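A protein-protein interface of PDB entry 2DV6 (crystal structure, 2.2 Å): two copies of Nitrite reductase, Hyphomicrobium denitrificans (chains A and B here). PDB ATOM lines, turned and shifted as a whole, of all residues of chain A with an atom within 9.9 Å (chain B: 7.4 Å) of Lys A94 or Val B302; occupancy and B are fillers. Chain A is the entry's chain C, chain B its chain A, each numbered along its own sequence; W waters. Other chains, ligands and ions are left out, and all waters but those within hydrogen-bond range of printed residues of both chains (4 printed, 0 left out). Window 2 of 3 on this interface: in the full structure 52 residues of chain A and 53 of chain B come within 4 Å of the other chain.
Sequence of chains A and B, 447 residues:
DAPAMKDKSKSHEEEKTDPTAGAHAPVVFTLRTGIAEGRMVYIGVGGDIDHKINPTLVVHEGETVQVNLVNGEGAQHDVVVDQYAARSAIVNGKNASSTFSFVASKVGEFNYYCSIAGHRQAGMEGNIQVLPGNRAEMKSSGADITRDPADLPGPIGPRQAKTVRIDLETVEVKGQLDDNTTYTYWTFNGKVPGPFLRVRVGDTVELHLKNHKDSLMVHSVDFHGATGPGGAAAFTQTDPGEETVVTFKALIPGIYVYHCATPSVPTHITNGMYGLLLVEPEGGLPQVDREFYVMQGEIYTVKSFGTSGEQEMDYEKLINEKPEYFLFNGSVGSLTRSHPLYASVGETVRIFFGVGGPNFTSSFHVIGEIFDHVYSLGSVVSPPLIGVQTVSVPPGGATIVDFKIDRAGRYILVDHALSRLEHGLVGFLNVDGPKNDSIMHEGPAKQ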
ATOM      1  N   ARG A  32       6.460 -33.850  21.873  1.00  0.00           N
ATOM      2  CA  ARG A  32       6.603 -34.475  20.554  1.00  0.00           C
ATOM      3  C   ARG A  32       5.297 -35.150  20.162  1.00  0.00           C
ATOM      4  O   ARG A  32       4.552 -35.639  21.012  1.00  0.00           O
ATOM      5  CB  ARG A  32       7.768 -35.494  20.480  1.00  0.00           C
ATOM      6  CG  ARG A  32       7.572 -36.739  21.328  1.00  0.00           C
ATOM      7  CD  ARG A  32       8.818 -37.716  21.331  1.00  0.00           C
ATOM      8  NE  ARG A  32       8.749 -38.682  22.459  1.00  0.00           N
ATOM      9  CZ  ARG A  32       8.070 -39.836  22.449  1.00  0.00           C
ATOM     10  NH1 ARG A  32       7.383 -40.199  21.366  1.00  0.00           N
ATOM     11  NH2 ARG A  32       8.075 -40.632  23.524  1.00  0.00           N
ATOM     12  N   THR A  33       4.997 -35.176  18.875  1.00  0.00           N
ATOM     13  CA  THR A  33       3.766 -35.819  18.459  1.00  0.00           C
ATOM     14  C   THR A  33       4.075 -37.306  18.192  1.00  0.00           C
ATOM     15  O   THR A  33       5.224 -37.684  17.902  1.00  0.00           O
ATOM     16  CB  THR A  33       3.172 -35.140  17.219  1.00  0.00           C
ATOM     17  OG1 THR A  33       3.995 -35.442  16.112  1.00  0.00           O
ATOM     18  CG2 THR A  33       3.143 -33.611  17.382  1.00  0.00           C
ATOM     19  N   GLY A  34       3.056 -38.141  18.321  1.00  0.00           N
ATOM     20  CA  GLY A  34       3.150 -39.513  17.925  1.00  0.00           C
ATOM     21  C   GLY A  34       1.861 -40.282  18.192  1.00  0.00           C
ATOM     22  O   GLY A  34       0.787 -39.705  18.368  1.00  0.00           O
ATOM     23  N   LEU A  69       7.435 -27.680  20.148  1.00  0.00           N
ATOM     24  CA  LEU A  69       6.753 -28.785  19.470  1.00  0.00           C
ATOM     25  C   LEU A  69       7.705 -29.455  18.479  1.00  0.00           C
ATOM     26  O   LEU A  69       8.250 -28.785  17.578  1.00  0.00           O
ATOM     27  CB  LEU A  69       5.618 -28.251  18.614  1.00  0.00           C
ATOM     28  CG  LEU A  69       4.351 -29.052  18.234  1.00  0.00           C
ATOM     29  CD1 LEU A  69       3.855 -28.910  16.833  1.00  0.00           C
ATOM     30  CD2 LEU A  69       4.137 -30.420  18.845  1.00  0.00           C
ATOM     31  N   VAL A  70       7.858 -30.765  18.583  1.00  0.00           N
ATOM     32  CA  VAL A  70       8.664 -31.479  17.592  1.00  0.00           C
ATOM     33  C   VAL A  70       7.794 -32.571  16.980  1.00  0.00           C
ATOM     34  O   VAL A  70       7.220 -33.372  17.697  1.00  0.00           O
ATOM     35  CB  VAL A  70       9.907 -32.118  18.238  1.00  0.00           C
ATOM     36  CG1 VAL A  70      10.746 -32.877  17.150  1.00  0.00           C
ATOM     37  CG2 VAL A  70      10.735 -31.037  19.013  1.00  0.00           C
ATOM     38  N   ASN A  71       7.710 -32.586  15.663  1.00  0.00           N
ATOM     39  CA  ASN A  71       6.939 -33.565  14.932  1.00  0.00           C
ATOM     40  C   ASN A  71       7.615 -34.946  15.036  1.00  0.00           C
ATOM     41  O   ASN A  71       8.790 -35.100  14.677  1.00  0.00           O
ATOM     42  CB  ASN A  71       6.815 -33.089  13.485  1.00  0.00           C
ATOM     43  CG  ASN A  71       5.977 -34.003  12.633  1.00  0.00           C
ATOM     44  OD1 ASN A  71       6.007 -35.210  12.793  1.00  0.00           O
ATOM     45  ND2 ASN A  71       5.255 -33.431  11.694  1.00  0.00           N
ATOM     46  N   GLY A  72       6.900 -35.932  15.572  1.00  0.00           N
ATOM     47  CA  GLY A  72       7.501 -37.242  15.833  1.00  0.00           C
ATOM     48  C   GLY A  72       7.314 -38.182  14.644  1.00  0.00           C
ATOM     49  O   GLY A  72       8.219 -38.903  14.274  1.00  0.00           O
ATOM     50  N   GLU A  73       6.156 -38.142  13.997  1.00  0.00           N
ATOM     51  CA  GLU A  73       5.791 -39.219  13.099  1.00  0.00           C
ATOM     52  C   GLU A  73       5.507 -38.784  11.650  1.00  0.00           C
ATOM     53  O   GLU A  73       5.417 -39.619  10.751  1.00  0.00           O
ATOM     54  CB  GLU A  73       4.684 -40.078  13.751  1.00  0.00           C
ATOM     55  CG  GLU A  73       3.237 -39.516  13.707  1.00  0.00           C
ATOM     56  CD  GLU A  73       3.142 -38.020  13.980  1.00  0.00           C
ATOM     57  OE1 GLU A  73       3.517 -37.572  15.069  1.00  0.00           O
ATOM     58  OE2 GLU A  73       2.707 -37.282  13.096  1.00  0.00           O
ATOM     59  N   GLY A  74       5.427 -37.479  11.391  1.00  0.00           N
ATOM     60  CA  GLY A  74       5.385 -37.017  10.014  1.00  0.00           C
ATOM     61  C   GLY A  74       4.049 -36.584   9.459  1.00  0.00           C
ATOM     62  O   GLY A  74       3.930 -36.299   8.259  1.00  0.00           O
ATOM     63  N   ALA A  75       3.023 -36.553  10.308  1.00  0.00           N
ATOM     64  CA  ALA A  75       1.761 -35.914   9.914  1.00  0.00           C
ATOM     65  C   ALA A  75       1.898 -34.420  10.234  1.00  0.00           C
ATOM     66  O   ALA A  75       2.797 -34.005  10.976  1.00  0.00           O
ATOM     67  CB  ALA A  75       0.588 -36.533  10.669  1.00  0.00           C
ATOM     68  N   GLN A  76       1.010 -33.614   9.697  1.00  0.00           N
ATOM     69  CA  GLN A  76       1.037 -32.185   9.893  1.00  0.00           C
ATOM     70  C   GLN A  76       0.437 -31.809  11.248  1.00  0.00           C
ATOM     71  O   GLN A  76      -0.617 -32.333  11.625  1.00  0.00           O
ATOM     72  CB  GLN A  76       0.274 -31.561   8.726  1.00  0.00           C
ATOM     73  CG  GLN A  76       0.537 -30.109   8.519  1.00  0.00           C
ATOM     74  CD  GLN A  76      -0.322 -29.542   7.415  1.00  0.00           C
ATOM     75  OE1 GLN A  76      -1.490 -29.913   7.271  1.00  0.00           O
ATOM     76  NE2 GLN A  76       0.252 -28.652   6.620  1.00  0.00           N
ATOM     77  N   HIS A  77       1.118 -30.946  12.013  1.00  0.00           N
ATOM     78  CA  HIS A  77       0.679 -30.615  13.379  1.00  0.00           C
ATOM     79  C   HIS A  77       0.945 -29.150  13.768  1.00  0.00           C
ATOM     80  O   HIS A  77       1.868 -28.503  13.246  1.00  0.00           O
ATOM     81  CB  HIS A  77       1.397 -31.487  14.450  1.00  0.00           C
ATOM     82  CG  HIS A  77       1.240 -32.955  14.255  1.00  0.00           C
ATOM     83  ND1 HIS A  77       0.010 -33.574  14.231  1.00  0.00           N
ATOM     84  CD2 HIS A  77       2.153 -33.932  14.041  1.00  0.00           C
ATOM     85  CE1 HIS A  77       0.167 -34.870  14.032  1.00  0.00           C
ATOM     86  NE2 HIS A  77       1.462 -35.113  13.925  1.00  0.00           N
ATOM     87  N   ILE A  90       2.855 -24.460  11.993  1.00  0.00           N
ATOM     88  CA  ILE A  90       2.574 -25.798  11.550  1.00  0.00           C
ATOM     89  C   ILE A  90       3.930 -26.439  11.143  1.00  0.00           C
ATOM     90  O   ILE A  90       4.801 -25.811  10.504  1.00  0.00           O
ATOM     91  CB  ILE A  90       1.606 -25.780  10.353  1.00  0.00           C
ATOM     92  CG1 ILE A  90       0.192 -25.361  10.783  1.00  0.00           C
ATOM     93  CG2 ILE A  90       1.559 -27.165   9.641  1.00  0.00           C
ATOM     94  CD1 ILE A  90      -0.619 -24.795   9.597  1.00  0.00           C
ATOM     95  N   VAL A  91       4.039 -27.711  11.489  1.00  0.00           N
ATOM     96  CA  VAL A  91       5.232 -28.520  11.413  1.00  0.00           C
ATOM     97  C   VAL A  91       4.855 -29.708  10.527  1.00  0.00           C
ATOM     98  O   VAL A  91       3.855 -30.378  10.756  1.00  0.00           O
ATOM     99  CB  VAL A  91       5.566 -28.767  12.900  1.00  0.00           C
ATOM    100  CG1 VAL A  91       5.364 -30.167  13.448  1.00  0.00           C
ATOM    101  CG2 VAL A  91       6.718 -27.915  13.399  1.00  0.00           C
ATOM    102  N   ASN A  92       5.607 -29.928   9.456  1.00  0.00           N
ATOM    103  CA  ASN A  92       5.163 -30.901   8.443  1.00  0.00           C
ATOM    104  C   ASN A  92       5.857 -32.270   8.435  1.00  0.00           C
ATOM    105  O   ASN A  92       5.190 -33.287   8.316  1.00  0.00           O
ATOM    106  CB  ASN A  92       5.190 -30.284   7.040  1.00  0.00           C
ATOM    107  CG  ASN A  92       4.244 -29.113   6.920  1.00  0.00           C
ATOM    108  OD1 ASN A  92       3.064 -29.316   6.736  1.00  0.00           O
ATOM    109  ND2 ASN A  92       4.759 -27.883   7.050  1.00  0.00           N
ATOM    110  N   GLY A  93       7.171 -32.327   8.493  1.00  0.00           N
ATOM    111  CA  GLY A  93       7.798 -33.655   8.427  1.00  0.00           C
ATOM    112  C   GLY A  93       8.372 -34.033   9.762  1.00  0.00           C
ATOM    113  O   GLY A  93       8.541 -33.176  10.651  1.00  0.00           O
ATOM    114  N   LYS A  94       8.720 -35.304   9.908  1.00  0.00           N
ATOM    115  CA  LYS A  94       9.401 -35.775  11.118  1.00  0.00           C
ATOM    116  C   LYS A  94      10.575 -34.863  11.495  1.00  0.00           C
ATOM    117  O   LYS A  94      11.373 -34.486  10.643  1.00  0.00           O
ATOM    118  CB  LYS A  94       9.906 -37.198  10.900  1.00  0.00           C
ATOM    119  CG  LYS A  94      10.380 -37.835  12.176  1.00  0.00           C
ATOM    120  CD  LYS A  94      10.594 -39.376  12.034  1.00  0.00           C
ATOM    121  CE  LYS A  94      11.133 -39.941  13.371  1.00  0.00           C
ATOM    122  NZ  LYS A  94      10.819 -41.415  13.558  1.00  0.00           N
ATOM    123  N   ASN A  95      10.661 -34.506  12.775  1.00  0.00           N
ATOM    124  CA  ASN A  95      11.730 -33.665  13.319  1.00  0.00           C
ATOM    125  C   ASN A  95      11.460 -32.182  13.181  1.00  0.00           C
ATOM    126  O   ASN A  95      12.056 -31.400  13.916  1.00  0.00           O
ATOM    127  CB  ASN A  95      13.134 -34.011  12.723  1.00  0.00           C
ATOM    128  CG  ASN A  95      13.638 -35.393  13.147  1.00  0.00           C
ATOM    129  OD1 ASN A  95      13.113 -35.994  14.073  1.00  0.00           O
ATOM    130  ND2 ASN A  95      14.660 -35.891  12.456  1.00  0.00           N
ATOM    131  N   ALA A  96      10.578 -31.794  12.264  1.00  0.00           N
ATOM    132  CA  ALA A  96      10.253 -30.385  12.050  1.00  0.00           C
ATOM    133  C   ALA A  96       9.736 -29.834  13.364  1.00  0.00           C
ATOM    134  O   ALA A  96       9.068 -30.548  14.121  1.00  0.00           O
ATOM    135  CB  ALA A  96       9.210 -30.211  10.921  1.00  0.00           C
ATOM    136  N   SER A  97      10.030 -28.575  13.643  1.00  0.00           N
ATOM    137  CA  SER A  97       9.853 -28.050  14.986  1.00  0.00           C
ATOM    138  C   SER A  97       9.350 -26.642  14.959  1.00  0.00           C
ATOM    139  O   SER A  97       9.626 -25.907  14.019  1.00  0.00           O
ATOM    140  CB  SER A  97      11.170 -28.047  15.750  1.00  0.00           C
ATOM    141  OG  SER A  97      11.755 -29.331  15.821  1.00  0.00           O
ATOM    142  N   SER A  98       8.567 -26.302  15.981  1.00  0.00           N
ATOM    143  CA  SER A  98       8.131 -24.940  16.239  1.00  0.00           C
ATOM    144  C   SER A  98       8.088 -24.635  17.735  1.00  0.00           C
ATOM    145  O   SER A  98       7.510 -25.361  18.555  1.00  0.00           O
ATOM    146  CB  SER A  98       6.790 -24.626  15.605  1.00  0.00           C
ATOM    147  OG  SER A  98       6.465 -23.285  15.923  1.00  0.00           O
ATOM    148  N   TYR B 183      12.216 -21.185   3.207  1.00  0.00           N
ATOM    149  CA  TYR B 183      12.264 -21.316   4.646  1.00  0.00           C
ATOM    150  C   TYR B 183      11.345 -20.198   5.152  1.00  0.00           C
ATOM    151  O   TYR B 183      11.259 -19.170   4.500  1.00  0.00           O
ATOM    152  CB  TYR B 183      13.724 -21.161   5.134  1.00  0.00           C
ATOM    153  CG  TYR B 183      13.922 -21.319   6.646  1.00  0.00           C
ATOM    154  CD1 TYR B 183      13.978 -22.581   7.233  1.00  0.00           C
ATOM    155  CD2 TYR B 183      14.096 -20.202   7.483  1.00  0.00           C
ATOM    156  CE1 TYR B 183      14.132 -22.732   8.611  1.00  0.00           C
ATOM    157  CE2 TYR B 183      14.282 -20.353   8.875  1.00  0.00           C
ATOM    158  CZ  TYR B 183      14.282 -21.630   9.419  1.00  0.00           C
ATOM    159  OH  TYR B 183      14.451 -21.822  10.773  1.00  0.00           O
ATOM    160  N   TYR B 300      18.940 -23.922  11.004  1.00  0.00           N
ATOM    161  CA  TYR B 300      18.982 -25.312  11.477  1.00  0.00           C
ATOM    162  C   TYR B 300      17.802 -26.064  10.866  1.00  0.00           C
ATOM    163  O   TYR B 300      16.741 -26.072  11.415  1.00  0.00           O
ATOM    164  CB  TYR B 300      18.919 -25.355  13.024  1.00  0.00           C
ATOM    165  CG  TYR B 300      20.073 -24.647  13.719  1.00  0.00           C
ATOM    166  CD1 TYR B 300      20.065 -23.252  13.891  1.00  0.00           C
ATOM    167  CD2 TYR B 300      21.178 -25.363  14.200  1.00  0.00           C
ATOM    168  CE1 TYR B 300      21.140 -22.575  14.512  1.00  0.00           C
ATOM    169  CE2 TYR B 300      22.244 -24.696  14.855  1.00  0.00           C
ATOM    170  CZ  TYR B 300      22.231 -23.308  14.984  1.00  0.00           C
ATOM    171  OH  TYR B 300      23.284 -22.662  15.628  1.00  0.00           O
ATOM    172  N   THR B 301      18.005 -26.693   9.722  1.00  0.00           N
ATOM    173  CA  THR B 301      16.910 -27.262   8.976  1.00  0.00           C
ATOM    174  C   THR B 301      16.874 -28.775   9.241  1.00  0.00           C
ATOM    175  O   THR B 301      17.879 -29.383   9.625  1.00  0.00           O
ATOM    176  CB  THR B 301      17.087 -27.013   7.488  1.00  0.00           C
ATOM    177  OG1 THR B 301      18.399 -27.405   7.131  1.00  0.00           O
ATOM    178  CG2 THR B 301      16.925 -25.555   7.139  1.00  0.00           C
ATOM    179  N   VAL B 302      15.700 -29.367   9.081  1.00  0.00           N
ATOM    180  CA  VAL B 302      15.522 -30.816   9.277  1.00  0.00           C
ATOM    181  C   VAL B 302      16.367 -31.580   8.244  1.00  0.00           C
ATOM    182  O   VAL B 302      17.072 -32.547   8.586  1.00  0.00           O
ATOM    183  CB  VAL B 302      14.027 -31.192   9.174  1.00  0.00           C
ATOM    184  CG1 VAL B 302      13.830 -32.746   9.148  1.00  0.00           C
ATOM    185  CG2 VAL B 302      13.273 -30.580  10.343  1.00  0.00           C
ATOM    186  N   LYS B 303      16.334 -31.126   6.998  1.00  0.00           N
ATOM    187  CA  LYS B 303      17.151 -31.769   5.951  1.00  0.00           C
ATOM    188  C   LYS B 303      18.532 -31.163   5.924  1.00  0.00           C
ATOM    189  O   LYS B 303      18.726 -30.009   6.367  1.00  0.00           O
ATOM    190  CB  LYS B 303      16.487 -31.631   4.567  1.00  0.00           C
ATOM    191  CG  LYS B 303      15.102 -32.276   4.472  1.00  0.00           C
ATOM    192  CD  LYS B 303      14.609 -32.194   2.996  1.00  0.00           C
ATOM    193  CE  LYS B 303      13.084 -32.076   2.827  1.00  0.00           C
ATOM    194  NZ  LYS B 303      12.402 -33.204   3.506  1.00  0.00           N
ATOM    195  N   SER B 304      19.488 -31.914   5.388  1.00  0.00           N
ATOM    196  CA  SER B 304      20.879 -31.430   5.285  1.00  0.00           C
ATOM    197  C   SER B 304      21.011 -30.247   4.321  1.00  0.00           C
ATOM    198  O   SER B 304      20.240 -30.134   3.379  1.00  0.00           O
ATOM    199  CB  SER B 304      21.808 -32.556   4.833  1.00  0.00           C
ATOM    200  OG  SER B 304      21.586 -33.708   5.639  1.00  0.00           O
ATOM    201  N   PHE B 305      21.995 -29.391   4.585  1.00  0.00           N
ATOM    202  CA  PHE B 305      22.419 -28.341   3.661  1.00  0.00           C
ATOM    203  C   PHE B 305      22.418 -28.890   2.241  1.00  0.00           C
ATOM    204  O   PHE B 305      22.964 -29.951   2.005  1.00  0.00           O
ATOM    205  CB  PHE B 305      23.862 -27.853   3.961  1.00  0.00           C
ATOM    206  CG  PHE B 305      24.367 -26.865   2.915  1.00  0.00           C
ATOM    207  CD1 PHE B 305      25.243 -27.263   1.908  1.00  0.00           C
ATOM    208  CD2 PHE B 305      23.890 -25.526   2.900  1.00  0.00           C
ATOM    209  CE1 PHE B 305      25.653 -26.334   0.898  1.00  0.00           C
ATOM    210  CE2 PHE B 305      24.288 -24.595   1.910  1.00  0.00           C
ATOM    211  CZ  PHE B 305      25.165 -24.978   0.909  1.00  0.00           C
ATOM    212  N   GLU B 310      10.970 -27.027   0.600  1.00  0.00           N
ATOM    213  CA  GLU B 310      10.535 -26.229   1.721  1.00  0.00           C
ATOM    214  C   GLU B 310      11.215 -26.709   2.996  1.00  0.00           C
ATOM    215  O   GLU B 310      11.005 -27.822   3.413  1.00  0.00           O
ATOM    216  CB  GLU B 310       9.011 -26.304   1.831  1.00  0.00           C
ATOM    217  CG  GLU B 310       8.330 -25.736   0.574  1.00  0.00           C
ATOM    218  CD  GLU B 310       6.868 -25.392   0.818  1.00  0.00           C
ATOM    219  OE1 GLU B 310       6.564 -24.285   1.369  1.00  0.00           O
ATOM    220  OE2 GLU B 310       6.031 -26.243   0.453  1.00  0.00           O
ATOM    221  N   GLN B 311      12.045 -25.875   3.596  1.00  0.00           N
ATOM    222  CA  GLN B 311      12.837 -26.302   4.739  1.00  0.00           C
ATOM    223  C   GLN B 311      12.126 -25.937   6.014  1.00  0.00           C
ATOM    224  O   GLN B 311      11.400 -24.929   6.063  1.00  0.00           O
ATOM    225  CB  GLN B 311      14.212 -25.654   4.712  1.00  0.00           C
ATOM    226  CG  GLN B 311      14.971 -25.892   3.456  1.00  0.00           C
ATOM    227  CD  GLN B 311      15.260 -27.352   3.202  1.00  0.00           C
ATOM    228  OE1 GLN B 311      15.032 -27.856   2.089  1.00  0.00           O
ATOM    229  NE2 GLN B 311      15.754 -28.045   4.210  1.00  0.00           N
ATOM    230  N   GLU B 312      12.343 -26.746   7.050  1.00  0.00           N
ATOM    231  CA  GLU B 312      11.727 -26.515   8.347  1.00  0.00           C
ATOM    232  C   GLU B 312      12.793 -26.509   9.425  1.00  0.00           C
ATOM    233  O   GLU B 312      13.852 -27.120   9.262  1.00  0.00           O
ATOM    234  CB  GLU B 312      10.695 -27.606   8.636  1.00  0.00           C
ATOM    235  CG  GLU B 312       9.682 -27.757   7.563  1.00  0.00           C
ATOM    236  CD  GLU B 312       8.521 -28.637   7.961  1.00  0.00           C
ATOM    237  OE1 GLU B 312       7.568 -28.121   8.598  1.00  0.00           O
ATOM    238  OE2 GLU B 312       8.570 -29.848   7.630  1.00  0.00           O
ATOM    239  N   MET B 313      12.516 -25.822  10.525  1.00  0.00           N
ATOM    240  CA  MET B 313      13.464 -25.698  11.619  1.00  0.00           C
ATOM    241  C   MET B 313      13.514 -27.028  12.348  1.00  0.00           C
ATOM    242  O   MET B 313      12.486 -27.674  12.549  1.00  0.00           O
ATOM    243  CB  MET B 313      13.015 -24.619  12.625  1.00  0.00           C
ATOM    244  CG  MET B 313      14.102 -24.312  13.623  1.00  0.00           C
ATOM    245  SD  MET B 313      13.656 -23.088  14.850  1.00  0.00           S
ATOM    246  CE  MET B 313      12.613 -24.056  15.950  1.00  0.00           C
ATOM    247  N   ASP B 314      14.705 -27.419  12.767  1.00  0.00           N
ATOM    248  CA  ASP B 314      14.873 -28.620  13.564  1.00  0.00           C
ATOM    249  C   ASP B 314      15.352 -28.108  14.938  1.00  0.00           C
ATOM    250  O   ASP B 314      16.468 -27.599  15.092  1.00  0.00           O
ATOM    251  CB  ASP B 314      15.896 -29.535  12.889  1.00  0.00           C
ATOM    252  CG  ASP B 314      16.148 -30.825  13.645  1.00  0.00           C
ATOM    253  OD1 ASP B 314      16.171 -30.814  14.905  1.00  0.00           O
ATOM    254  OD2 ASP B 314      16.367 -31.857  12.961  1.00  0.00           O
ATOM    255  N   TYR B 315      14.474 -28.233  15.924  1.00  0.00           N
ATOM    256  CA  TYR B 315      14.774 -27.799  17.290  1.00  0.00           C
ATOM    257  C   TYR B 315      15.963 -28.520  17.945  1.00  0.00           C
ATOM    258  O   TYR B 315      16.769 -27.879  18.604  1.00  0.00           O
ATOM    259  CB  TYR B 315      13.512 -27.902  18.158  1.00  0.00           C
ATOM    260  CG  TYR B 315      13.776 -27.767  19.620  1.00  0.00           C
ATOM    261  CD1 TYR B 315      13.869 -26.521  20.230  1.00  0.00           C
ATOM    262  CD2 TYR B 315      13.939 -28.913  20.406  1.00  0.00           C
ATOM    263  CE1 TYR B 315      14.128 -26.431  21.628  1.00  0.00           C
ATOM    264  CE2 TYR B 315      14.201 -28.834  21.745  1.00  0.00           C
ATOM    265  CZ  TYR B 315      14.278 -27.603  22.353  1.00  0.00           C
ATOM    266  OH  TYR B 315      14.539 -27.610  23.705  1.00  0.00           O
ATOM    267  N   LYS B 317      18.557 -29.756  16.479  1.00  0.00           N
ATOM    268  CA  LYS B 317      19.789 -29.221  15.882  1.00  0.00           C
ATOM    269  C   LYS B 317      20.076 -27.817  16.410  1.00  0.00           C
ATOM    270  O   LYS B 317      21.218 -27.510  16.729  1.00  0.00           O
ATOM    271  CB  LYS B 317      19.718 -29.214  14.348  1.00  0.00           C
ATOM    272  CG  LYS B 317      19.872 -30.598  13.683  1.00  0.00           C
ATOM    273  CD  LYS B 317      19.679 -30.424  12.140  1.00  0.00           C
ATOM    274  CE  LYS B 317      19.616 -31.796  11.387  1.00  0.00           C
ATOM    275  NZ  LYS B 317      19.760 -31.532   9.892  1.00  0.00           N
ATOM    276  N   GLU B 324      22.889 -26.238   9.755  1.00  0.00           N
ATOM    277  CA  GLU B 324      22.969 -26.739   8.393  1.00  0.00           C
ATOM    278  C   GLU B 324      23.415 -25.649   7.430  1.00  0.00           C
ATOM    279  O   GLU B 324      24.091 -25.937   6.449  1.00  0.00           O
ATOM    280  CB  GLU B 324      21.614 -27.300   7.944  1.00  0.00           C
ATOM    281  CG  GLU B 324      21.236 -28.574   8.696  1.00  0.00           C
ATOM    282  CD  GLU B 324      22.161 -29.766   8.356  1.00  0.00           C
ATOM    283  OE1 GLU B 324      22.861 -29.737   7.326  1.00  0.00           O
ATOM    284  OE2 GLU B 324      22.198 -30.727   9.129  1.00  0.00           O
ATOM    285  N   TYR B 325      22.972 -24.418   7.674  1.00  0.00           N
ATOM    286  CA  TYR B 325      23.293 -23.282   6.824  1.00  0.00           C
ATOM    287  C   TYR B 325      24.003 -22.231   7.651  1.00  0.00           C
ATOM    288  O   TYR B 325      23.597 -21.958   8.784  1.00  0.00           O
ATOM    289  CB  TYR B 325      22.031 -22.674   6.213  1.00  0.00           C
ATOM    290  CG  TYR B 325      21.335 -23.574   5.191  1.00  0.00           C
ATOM    291  CD1 TYR B 325      20.476 -24.597   5.594  1.00  0.00           C
ATOM    292  CD2 TYR B 325      21.530 -23.379   3.816  1.00  0.00           C
ATOM    293  CE1 TYR B 325      19.847 -25.425   4.642  1.00  0.00           C
ATOM    294  CE2 TYR B 325      20.926 -24.198   2.877  1.00  0.00           C
ATOM    295  CZ  TYR B 325      20.092 -25.198   3.275  1.00  0.00           C
ATOM    296  OH  TYR B 325      19.495 -25.976   2.308  1.00  0.00           O
HETATM  297  O   HOH W   1      13.956 -31.834  15.954  1.00  0.00           O
HETATM  298  O   HOH W   2       9.481 -24.938  11.318  1.00  0.00           O
HETATM  299  O   HOH W   3       7.434 -25.867   9.817  1.00  0.00           O
HETATM  300  O   HOH W   4      16.497 -33.772  11.034  1.00  0.00           O
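Among the printed residues, 13 pairs touch across the chains. Among the printed residues, no Asp or Glu carboxylate lies within 4 Å of a Lys or Arg side-chain nitrogen of the other chain.
Among the printed residues, merely in contact across the chains: Val A91 with Glu B312, Lys A94 with Val B302, Asn A95 with Val B302, Asn A95 with Met B313, Asn A95 with Asp B314, Ala A96 with Val B302, Ala A96 with Glu B312, Ala A96 with Met B313 and Ser A97 with Asp B314.
Water W3 bridges the side-chain carboxylate of Glu B312 and the backbone carbonyl oxygen of Ile A90. Water W1 lies within hydrogen-bond range of OD1 of Asp B314, O of Asn A95 and OG of Ser A97. Water W4 lies within hydrogen-bond range of the side-chain carboxylate (OD2) of Asp B314 (2.7 Å), the backbone carbonyl oxygen (O) of Val B302 (2.8 Å) and the side-chain amide nitrogen (ND2) of Asn A95 (3.1 Å). Water W2 bridges the backbone carbonyl oxygen (O) of Ser A97 (2.9 Å) and the backbone NH (N) of Met B313 (3.3 Å).
Printed residues of chain B within 4 Å of Val A91: Glu B312. Lys A94 touches one residue of chain B. Of the printed residues of chain B, Ala A96 touches Val B302 (3.5 Å), Glu B312 (3.4 Å) and Met B313 (3.5 Å). No residue of chain A comes within 4 Å of Thr B301. Val B302 touches just these residues of chain A: Lys A94, Asn A95 and Ala A96. Of the printed residues of chain A, Glu B312 touches Val A91 (3.7 Å), Asn A92 (2.8 Å), Gly A93 (3.0 Å) and Ala A96 (3.4 Å). Of the printed residues of chain A, Met B313 touches Asn A95 (3.99 Å), Ala A96 (3.5 Å) and Ser A97 (2.8 Å). Of the printed residues of chain A, Tyr B315 touches Ser A97.
No position is printed for both chains. Of the 13 pairs that touch across the chains among the printed residues, none has its exchanged pair printed and touching as well.
OE2 of Glu B312 lies within hydrogen-bond range of N of Gly A93, at 3.0 Å. The side-chain carboxylate of Glu B312 is in hydrogen-bond range of the backbone NH of Asn A92, at 2.8 Å. N of Tyr B315 sits at hydrogen-bond distance from OG of Ser A97 (2.9 Å). The backbone NH (N) of Ser A97 lies within hydrogen-bond range of the backbone carbonyl oxygen (O) of Met B313, 2.8 Å away.
The backbone carbonyl oxygen (O) of Asn A71 lies within hydrogen-bond range of the backbone NH (N) of Asn A95 (2.7 Å). The backbone NH of Asp B314 sits at hydrogen-bond distance from the backbone carbonyl oxygen of Tyr B300 (2.8 Å). The backbone carbonyl oxygen (O) of Gly A93 lies close to the side-chain amide nitrogen (ND2) of Asn A71 (3.5 Å). The backbone NH (N) of Val B302 sits at hydrogen-bond distance from the backbone carbonyl oxygen (O) of Glu B312 (2.9 Å). The side-chain hydroxyl (OG) of Ser A97 lies within hydrogen-bond range of the backbone carbonyl oxygen (O) of Asn A95, 2.8 Å away. ND2 of Asn A71 lies within hydrogen-bond range of O of Val A91 (3.5 Å).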
